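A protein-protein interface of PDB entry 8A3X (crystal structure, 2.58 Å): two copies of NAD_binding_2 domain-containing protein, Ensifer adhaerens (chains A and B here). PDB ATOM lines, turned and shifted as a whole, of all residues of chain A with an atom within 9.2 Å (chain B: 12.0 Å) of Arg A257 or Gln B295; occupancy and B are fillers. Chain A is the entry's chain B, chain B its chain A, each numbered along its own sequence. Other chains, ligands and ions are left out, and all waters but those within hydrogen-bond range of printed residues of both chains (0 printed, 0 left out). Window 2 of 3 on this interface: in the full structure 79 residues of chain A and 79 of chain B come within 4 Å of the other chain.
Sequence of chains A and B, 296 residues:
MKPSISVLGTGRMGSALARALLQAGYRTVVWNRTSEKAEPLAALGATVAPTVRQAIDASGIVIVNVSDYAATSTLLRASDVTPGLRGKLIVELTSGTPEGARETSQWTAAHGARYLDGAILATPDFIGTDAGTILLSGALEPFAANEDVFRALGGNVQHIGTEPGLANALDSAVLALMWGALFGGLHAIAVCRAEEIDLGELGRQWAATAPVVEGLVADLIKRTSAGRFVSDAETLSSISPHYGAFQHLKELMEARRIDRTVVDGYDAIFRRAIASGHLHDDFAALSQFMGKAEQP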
ATOM      1  N   ALA A 190     -11.651  12.424 -21.617  1.00  0.00           N
ATOM      2  CA  ALA A 190     -11.321  10.994 -21.395  1.00  0.00           C
ATOM      3  C   ALA A 190     -10.120  10.889 -20.450  1.00  0.00           C
ATOM      4  O   ALA A 190     -10.128  10.004 -19.582  1.00  0.00           O
ATOM      5  CB  ALA A 190     -11.061  10.299 -22.700  1.00  0.00           C
ATOM      6  N   ALA A 194      -9.975   9.535 -16.478  1.00  0.00           N
ATOM      7  CA  ALA A 194      -8.965   8.508 -16.128  1.00  0.00           C
ATOM      8  C   ALA A 194      -8.120   8.941 -14.923  1.00  0.00           C
ATOM      9  O   ALA A 194      -7.792   8.057 -14.113  1.00  0.00           O
ATOM     10  CB  ALA A 194      -8.086   8.232 -17.322  1.00  0.00           C
ATOM     11  N   LEU A 249       0.757  11.395 -23.575  1.00  0.00           N
ATOM     12  CA  LEU A 249      -0.693  11.287 -23.903  1.00  0.00           C
ATOM     13  C   LEU A 249      -0.995   9.914 -24.517  1.00  0.00           C
ATOM     14  O   LEU A 249      -1.962   9.253 -24.038  1.00  0.00           O
ATOM     15  CB  LEU A 249      -1.080  12.419 -24.861  1.00  0.00           C
ATOM     16  CG  LEU A 249      -2.506  12.384 -25.411  1.00  0.00           C
ATOM     17  CD1 LEU A 249      -3.533  12.308 -24.295  1.00  0.00           C
ATOM     18  CD2 LEU A 249      -2.761  13.586 -26.294  1.00  0.00           C
ATOM     19  N   LYS A 250      -0.228   9.510 -25.543  1.00  0.00           N
ATOM     20  CA  LYS A 250      -0.345   8.171 -26.181  1.00  0.00           C
ATOM     21  C   LYS A 250      -0.290   7.074 -25.111  1.00  0.00           C
ATOM     22  O   LYS A 250      -1.219   6.227 -25.085  1.00  0.00           O
ATOM     23  CB  LYS A 250       0.803   7.891 -27.149  1.00  0.00           C
ATOM     24  CG  LYS A 250       0.552   8.229 -28.597  1.00  0.00           C
ATOM     25  CD  LYS A 250       1.655   7.729 -29.504  1.00  0.00           C
ATOM     26  CE  LYS A 250       2.983   8.441 -29.292  1.00  0.00           C
ATOM     27  NZ  LYS A 250       4.062   7.782 -30.067  1.00  0.00           N
ATOM     28  N   GLU A 251       0.772   7.082 -24.288  1.00  0.00           N
ATOM     29  CA  GLU A 251       1.009   6.062 -23.233  1.00  0.00           C
ATOM     30  C   GLU A 251      -0.235   6.020 -22.336  1.00  0.00           C
ATOM     31  O   GLU A 251      -0.730   4.910 -22.082  1.00  0.00           O
ATOM     32  CB  GLU A 251       2.311   6.331 -22.460  1.00  0.00           C
ATOM     33  CG  GLU A 251       3.595   5.983 -23.223  1.00  0.00           C
ATOM     34  N   LEU A 252      -0.744   7.184 -21.916  1.00  0.00           N
ATOM     35  CA  LEU A 252      -1.921   7.306 -21.006  1.00  0.00           C
ATOM     36  C   LEU A 252      -3.147   6.652 -21.655  1.00  0.00           C
ATOM     37  O   LEU A 252      -3.870   5.910 -20.958  1.00  0.00           O
ATOM     38  CB  LEU A 252      -2.172   8.788 -20.704  1.00  0.00           C
ATOM     39  CG  LEU A 252      -3.410   9.096 -19.864  1.00  0.00           C
ATOM     40  CD1 LEU A 252      -3.329   8.374 -18.533  1.00  0.00           C
ATOM     41  CD2 LEU A 252      -3.571  10.590 -19.672  1.00  0.00           C
ATOM     42  N   MET A 253      -3.372   6.928 -22.943  1.00  0.00           N
ATOM     43  CA  MET A 253      -4.560   6.435 -23.685  1.00  0.00           C
ATOM     44  C   MET A 253      -4.432   4.923 -23.912  1.00  0.00           C
ATOM     45  O   MET A 253      -5.443   4.206 -23.711  1.00  0.00           O
ATOM     46  CB  MET A 253      -4.728   7.192 -25.001  1.00  0.00           C
ATOM     47  CG  MET A 253      -5.512   8.513 -24.825  1.00  0.00           C
ATOM     48  SD  MET A 253      -5.783   9.389 -26.392  1.00  0.00           S
ATOM     49  CE  MET A 253      -4.094   9.870 -26.731  1.00  0.00           C
ATOM     50  N   GLU A 254      -3.240   4.449 -24.295  1.00  0.00           N
ATOM     51  CA  GLU A 254      -2.936   2.991 -24.417  1.00  0.00           C
ATOM     52  C   GLU A 254      -3.292   2.294 -23.096  1.00  0.00           C
ATOM     53  O   GLU A 254      -4.027   1.294 -23.130  1.00  0.00           O
ATOM     54  CB  GLU A 254      -1.469   2.778 -24.795  1.00  0.00           C
ATOM     55  CG  GLU A 254      -1.033   1.319 -24.819  1.00  0.00           C
ATOM     56  CD  GLU A 254      -1.713   0.416 -25.835  1.00  0.00           C
ATOM     57  OE1 GLU A 254      -1.801  -0.792 -25.553  1.00  0.00           O
ATOM     58  OE2 GLU A 254      -2.160   0.922 -26.898  1.00  0.00           O
ATOM     59  N   ALA A 255      -2.797   2.830 -21.983  1.00  0.00           N
ATOM     60  CA  ALA A 255      -2.953   2.269 -20.621  1.00  0.00           C
ATOM     61  C   ALA A 255      -4.428   2.261 -20.215  1.00  0.00           C
ATOM     62  O   ALA A 255      -4.836   1.307 -19.534  1.00  0.00           O
ATOM     63  CB  ALA A 255      -2.123   3.062 -19.643  1.00  0.00           C
ATOM     64  N   ARG A 256      -5.191   3.289 -20.604  1.00  0.00           N
ATOM     65  CA  ARG A 256      -6.582   3.511 -20.122  1.00  0.00           C
ATOM     66  C   ARG A 256      -7.603   3.008 -21.151  1.00  0.00           C
ATOM     67  O   ARG A 256      -8.803   3.267 -20.940  1.00  0.00           O
ATOM     68  CB  ARG A 256      -6.789   4.991 -19.794  1.00  0.00           C
ATOM     69  CG  ARG A 256      -6.006   5.497 -18.591  1.00  0.00           C
ATOM     70  CD  ARG A 256      -6.300   4.740 -17.304  1.00  0.00           C
ATOM     71  NE  ARG A 256      -5.542   5.253 -16.167  1.00  0.00           N
ATOM     72  CZ  ARG A 256      -5.952   5.230 -14.898  1.00  0.00           C
ATOM     73  NH1 ARG A 256      -7.124   4.698 -14.579  1.00  0.00           N
ATOM     74  NH2 ARG A 256      -5.167   5.734 -13.955  1.00  0.00           N
ATOM     75  N   ARG A 257      -7.161   2.290 -22.193  1.00  0.00           N
ATOM     76  CA  ARG A 257      -8.035   1.684 -23.240  1.00  0.00           C
ATOM     77  C   ARG A 257      -8.923   2.773 -23.878  1.00  0.00           C
ATOM     78  O   ARG A 257     -10.148   2.541 -24.054  1.00  0.00           O
ATOM     79  CB  ARG A 257      -8.884   0.555 -22.644  1.00  0.00           C
ATOM     80  CG  ARG A 257      -8.278  -0.837 -22.744  1.00  0.00           C
ATOM     81  CD  ARG A 257      -9.299  -1.823 -22.223  1.00  0.00           C
ATOM     82  NE  ARG A 257     -10.494  -1.885 -23.057  1.00  0.00           N
ATOM     83  CZ  ARG A 257     -10.699  -2.750 -24.045  1.00  0.00           C
ATOM     84  NH1 ARG A 257      -9.803  -3.679 -24.339  1.00  0.00           N
ATOM     85  NH2 ARG A 257     -11.834  -2.703 -24.721  1.00  0.00           N
ATOM     86  N   ILE A 258      -8.324   3.921 -24.206  1.00  0.00           N
ATOM     87  CA  ILE A 258      -8.965   5.041 -24.960  1.00  0.00           C
ATOM     88  C   ILE A 258      -8.579   4.893 -26.437  1.00  0.00           C
ATOM     89  O   ILE A 258      -7.381   4.704 -26.707  1.00  0.00           O
ATOM     90  CB  ILE A 258      -8.550   6.406 -24.366  1.00  0.00           C
ATOM     91  CG1 ILE A 258      -9.137   6.608 -22.965  1.00  0.00           C
ATOM     92  CG2 ILE A 258      -8.944   7.539 -25.302  1.00  0.00           C
ATOM     93  CD1 ILE A 258      -8.670   7.877 -22.257  1.00  0.00           C
ATOM     94  N   ASP A 259      -9.553   4.970 -27.350  1.00  0.00           N
ATOM     95  CA  ASP A 259      -9.349   4.780 -28.812  1.00  0.00           C
ATOM     96  C   ASP A 259      -8.210   5.702 -29.254  1.00  0.00           C
ATOM     97  O   ASP A 259      -8.256   6.921 -28.948  1.00  0.00           O
ATOM     98  CB  ASP A 259     -10.627   5.046 -29.609  1.00  0.00           C
ATOM     99  CG  ASP A 259     -10.529   4.714 -31.091  1.00  0.00           C
ATOM    100  OD1 ASP A 259     -10.598   3.529 -31.411  1.00  0.00           O
ATOM    101  OD2 ASP A 259     -10.404   5.655 -31.915  1.00  0.00           O
ATOM    102  N   ARG A 260      -7.222   5.122 -29.924  1.00  0.00           N
ATOM    103  CA  ARG A 260      -5.963   5.809 -30.300  1.00  0.00           C
ATOM    104  C   ARG A 260      -5.976   6.129 -31.789  1.00  0.00           C
ATOM    105  O   ARG A 260      -4.945   6.650 -32.287  1.00  0.00           O
ATOM    106  CB  ARG A 260      -4.773   4.901 -29.979  1.00  0.00           C
ATOM    107  CG  ARG A 260      -4.562   4.645 -28.497  1.00  0.00           C
ATOM    108  CD  ARG A 260      -3.225   3.975 -28.252  1.00  0.00           C
ATOM    109  NE  ARG A 260      -2.116   4.647 -28.925  1.00  0.00           N
ATOM    110  CZ  ARG A 260      -0.910   4.127 -29.119  1.00  0.00           C
ATOM    111  NH1 ARG A 260      -0.634   2.904 -28.696  1.00  0.00           N
ATOM    112  NH2 ARG A 260       0.004   4.838 -29.764  1.00  0.00           N
ATOM    113  N   ILE B 269     -16.018   7.461 -34.125  1.00  0.00           N
ATOM    114  CA  ILE B 269     -16.673   7.933 -32.868  1.00  0.00           C
ATOM    115  C   ILE B 269     -18.118   8.328 -33.199  1.00  0.00           C
ATOM    116  O   ILE B 269     -19.041   7.842 -32.516  1.00  0.00           O
ATOM    117  CB  ILE B 269     -15.872   9.088 -32.225  1.00  0.00           C
ATOM    118  CG1 ILE B 269     -14.453   8.656 -31.849  1.00  0.00           C
ATOM    119  CG2 ILE B 269     -16.609   9.662 -31.028  1.00  0.00           C
ATOM    120  CD1 ILE B 269     -13.491   9.797 -31.673  1.00  0.00           C
ATOM    121  N   ARG B 272     -20.180   5.168 -33.903  1.00  0.00           N
ATOM    122  CA  ARG B 272     -20.417   4.485 -32.601  1.00  0.00           C
ATOM    123  C   ARG B 272     -21.595   5.173 -31.886  1.00  0.00           C
ATOM    124  O   ARG B 272     -22.466   4.478 -31.331  1.00  0.00           O
ATOM    125  CB  ARG B 272     -19.134   4.531 -31.761  1.00  0.00           C
ATOM    126  CG  ARG B 272     -18.647   3.204 -31.196  1.00  0.00           C
ATOM    127  CD  ARG B 272     -17.348   3.378 -30.425  1.00  0.00           C
ATOM    128  NE  ARG B 272     -16.175   3.394 -31.296  1.00  0.00           N
ATOM    129  CZ  ARG B 272     -15.103   4.169 -31.133  1.00  0.00           C
ATOM    130  NH1 ARG B 272     -15.057   5.048 -30.155  1.00  0.00           N
ATOM    131  NH2 ARG B 272     -14.079   4.093 -31.963  1.00  0.00           N
ATOM    132  N   ALA B 275     -24.830   4.490 -33.903  1.00  0.00           N
ATOM    133  CA  ALA B 275     -25.189   3.064 -33.720  1.00  0.00           C
ATOM    134  C   ALA B 275     -26.054   2.873 -32.463  1.00  0.00           C
ATOM    135  O   ALA B 275     -26.976   2.045 -32.497  1.00  0.00           O
ATOM    136  CB  ALA B 275     -23.945   2.219 -33.669  1.00  0.00           C
ATOM    137  N   SER B 276     -25.759   3.585 -31.370  1.00  0.00           N
ATOM    138  CA  SER B 276     -26.746   3.868 -30.292  1.00  0.00           C
ATOM    139  C   SER B 276     -27.656   4.995 -30.796  1.00  0.00           C
ATOM    140  O   SER B 276     -27.253   5.698 -31.736  1.00  0.00           O
ATOM    141  CB  SER B 276     -26.069   4.206 -29.011  1.00  0.00           C
ATOM    142  OG  SER B 276     -24.866   3.443 -28.892  1.00  0.00           O
ATOM    143  N   LEU B 286     -21.160  12.149 -27.858  1.00  0.00           N
ATOM    144  CA  LEU B 286     -19.908  11.531 -28.388  1.00  0.00           C
ATOM    145  C   LEU B 286     -18.959  11.153 -27.240  1.00  0.00           C
ATOM    146  O   LEU B 286     -18.222  10.188 -27.399  1.00  0.00           O
ATOM    147  CB  LEU B 286     -19.209  12.488 -29.356  1.00  0.00           C
ATOM    148  CG  LEU B 286     -19.939  12.782 -30.664  1.00  0.00           C
ATOM    149  CD1 LEU B 286     -19.066  13.637 -31.575  1.00  0.00           C
ATOM    150  CD2 LEU B 286     -20.350  11.510 -31.359  1.00  0.00           C
ATOM    151  N   SER B 287     -18.977  11.877 -26.121  1.00  0.00           N
ATOM    152  CA  SER B 287     -18.078  11.669 -24.955  1.00  0.00           C
ATOM    153  C   SER B 287     -18.233  10.250 -24.382  1.00  0.00           C
ATOM    154  O   SER B 287     -17.236   9.748 -23.806  1.00  0.00           O
ATOM    155  CB  SER B 287     -18.297  12.719 -23.908  1.00  0.00           C
ATOM    156  OG  SER B 287     -19.559  12.573 -23.266  1.00  0.00           O
ATOM    157  N   GLN B 288     -19.391   9.601 -24.575  1.00  0.00           N
ATOM    158  CA  GLN B 288     -19.642   8.214 -24.085  1.00  0.00           C
ATOM    159  C   GLN B 288     -19.008   7.146 -24.996  1.00  0.00           C
ATOM    160  O   GLN B 288     -19.162   5.945 -24.691  1.00  0.00           O
ATOM    161  CB  GLN B 288     -21.136   7.892 -24.040  1.00  0.00           C
ATOM    162  CG  GLN B 288     -22.004   8.858 -23.263  1.00  0.00           C
ATOM    163  CD  GLN B 288     -23.462   8.557 -23.515  1.00  0.00           C
ATOM    164  OE1 GLN B 288     -23.991   8.900 -24.559  1.00  0.00           O
ATOM    165  NE2 GLN B 288     -24.125   7.917 -22.564  1.00  0.00           N
ATOM    166  N   PHE B 289     -18.381   7.538 -26.108  1.00  0.00           N
ATOM    167  CA  PHE B 289     -17.922   6.604 -27.169  1.00  0.00           C
ATOM    168  C   PHE B 289     -16.459   6.874 -27.465  1.00  0.00           C
ATOM    169  O   PHE B 289     -16.064   6.892 -28.636  1.00  0.00           O
ATOM    170  CB  PHE B 289     -18.794   6.764 -28.406  1.00  0.00           C
ATOM    171  CG  PHE B 289     -20.237   6.498 -28.094  1.00  0.00           C
ATOM    172  CD1 PHE B 289     -20.685   5.209 -27.858  1.00  0.00           C
ATOM    173  CD2 PHE B 289     -21.117   7.554 -27.930  1.00  0.00           C
ATOM    174  CE1 PHE B 289     -22.005   4.979 -27.517  1.00  0.00           C
ATOM    175  CE2 PHE B 289     -22.444   7.317 -27.616  1.00  0.00           C
ATOM    176  CZ  PHE B 289     -22.882   6.034 -27.405  1.00  0.00           C
ATOM    177  N   MET B 290     -15.689   7.038 -26.397  1.00  0.00           N
ATOM    178  CA  MET B 290     -14.280   7.479 -26.450  1.00  0.00           C
ATOM    179  C   MET B 290     -13.355   6.280 -26.201  1.00  0.00           C
ATOM    180  O   MET B 290     -12.168   6.382 -26.587  1.00  0.00           O
ATOM    181  CB  MET B 290     -14.056   8.563 -25.392  1.00  0.00           C
ATOM    182  CG  MET B 290     -13.413   9.795 -25.954  1.00  0.00           C
ATOM    183  SD  MET B 290     -14.249  10.285 -27.453  1.00  0.00           S
ATOM    184  CE  MET B 290     -12.837  10.596 -28.508  1.00  0.00           C
ATOM    185  N   GLY B 291     -13.890   5.201 -25.601  1.00  0.00           N
ATOM    186  CA  GLY B 291     -13.162   3.956 -25.273  1.00  0.00           C
ATOM    187  C   GLY B 291     -12.848   3.129 -26.510  1.00  0.00           C
ATOM    188  O   GLY B 291     -13.448   3.402 -27.554  1.00  0.00           O
ATOM    189  N   LYS B 292     -11.969   2.131 -26.394  1.00  0.00           N
ATOM    190  CA  LYS B 292     -11.462   1.336 -27.548  1.00  0.00           C
ATOM    191  C   LYS B 292     -12.611   0.479 -28.085  1.00  0.00           C
ATOM    192  O   LYS B 292     -13.536   0.202 -27.308  1.00  0.00           O
ATOM    193  CB  LYS B 292     -10.246   0.488 -27.165  1.00  0.00           C
ATOM    194  CG  LYS B 292      -9.188   0.389 -28.257  1.00  0.00           C
ATOM    195  CD  LYS B 292      -8.139  -0.675 -28.021  1.00  0.00           C
ATOM    196  CE  LYS B 292      -6.951  -0.500 -28.944  1.00  0.00           C
ATOM    197  NZ  LYS B 292      -5.941  -1.566 -28.763  1.00  0.00           N
ATOM    198  N   ALA B 293     -12.609   0.162 -29.379  1.00  0.00           N
ATOM    199  CA  ALA B 293     -13.762  -0.465 -30.059  1.00  0.00           C
ATOM    200  C   ALA B 293     -13.792  -1.967 -29.745  1.00  0.00           C
ATOM    201  O   ALA B 293     -14.784  -2.421 -29.146  1.00  0.00           O
ATOM    202  CB  ALA B 293     -13.682  -0.173 -31.529  1.00  0.00           C
ATOM    203  N   GLU B 294     -12.741  -2.703 -30.125  1.00  0.00           N
ATOM    204  CA  GLU B 294     -12.531  -4.148 -29.802  1.00  0.00           C
ATOM    205  C   GLU B 294     -12.489  -4.312 -28.278  1.00  0.00           C
ATOM    206  O   GLU B 294     -12.125  -3.333 -27.606  1.00  0.00           O
ATOM    207  CB  GLU B 294     -11.242  -4.686 -30.440  1.00  0.00           C
ATOM    208  CG  GLU B 294     -10.029  -3.777 -30.263  1.00  0.00           C
ATOM    209  CD  GLU B 294      -9.847  -2.723 -31.346  1.00  0.00           C
ATOM    210  OE1 GLU B 294      -9.626  -3.113 -32.508  1.00  0.00           O
ATOM    211  OE2 GLU B 294      -9.950  -1.512 -31.032  1.00  0.00           O
ATOM    212  N   GLN B 295     -12.787  -5.512 -27.765  1.00  0.00           N
ATOM    213  CA  GLN B 295     -13.099  -5.764 -26.325  1.00  0.00           C
ATOM    214  C   GLN B 295     -12.453  -7.076 -25.837  1.00  0.00           C
ATOM    215  O   GLN B 295     -12.469  -7.408 -24.642  1.00  0.00           O
ATOM    216  CB  GLN B 295     -14.623  -5.733 -26.166  1.00  0.00           C
ATOM    217  CG  GLN B 295     -15.390  -5.730 -27.494  1.00  0.00           C
ATOM    218  CD  GLN B 295     -16.878  -5.487 -27.342  1.00  0.00           C
ATOM    219  OE1 GLN B 295     -17.702  -6.041 -28.076  1.00  0.00           O
ATOM    220  NE2 GLN B 295     -17.236  -4.640 -26.387  1.00  0.00           N
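Glu A251 touches none of the printed residues of chain B.
No residue of chain B comes within 4 Å of Glu A254.
No residue of chain B comes within 4 Å of Ala A255.
Arg A257 touches just these residues of chain B: Gly B291, Lys B292, Glu B294 and Gln B295.
Ile A258 touches one residue of chain B.
Printed residues of chain B within 4 Å of Asp A259: Arg B272, Met B290, Gly B291 and Lys B292.
Of the printed residues of chain A, Met B290 touches Ile A258 and Asp A259.
Of chain A, only Arg A257 comes within 4 Å of Gln B295.
The nearest printed residue of chain B that does not touch Asp A259 is Ala B293 (4.4 Å).
No position is printed for both chains.
O of Arg A257 touches CA of Gly B291, at 3.5 Å.
Gln B295 touches Arg A257 (CA to NH2, 3.7 Å).
Ile A258 touches Met B290.
Gly B291 touches Asp A259.
Asp A259 touches Lys B292 (N to N, 3.8 Å).
O of Phe B289 lies within hydrogen-bond range of NH1 of Arg B272 (2.6 Å).
The backbone carbonyl oxygen (O) of Met A253 sits at hydrogen-bond distance from the backbone NH (N) of Ile A258, at 2.9 Å.
The guanidinium group (NH1) of Arg B272 lies within hydrogen-bond range of the backbone carbonyl oxygen (O) of Gly B291 (3.5 Å).
O of Met B290 is in hydrogen-bond range of N of Asp A259 (3.1 Å).
The guanidinium group (NH2) of Arg B272 is in salt-bridge range of the side-chain carboxylate (OD1) of Asp A259 (3.6 Å).
NH2 of Arg A257 is in hydrogen-bond range of O of Glu B294 (3.0 Å).
N of Lys B292 lies within hydrogen-bond range of O of Arg A257, at 3.0 Å.
Printed residues of chain A that touch a printed residue of chain B: Arg A257, Ile A258 and Asp A259.
Of the 14 printed residues of chain B, 6 touch a printed residue of chain A.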
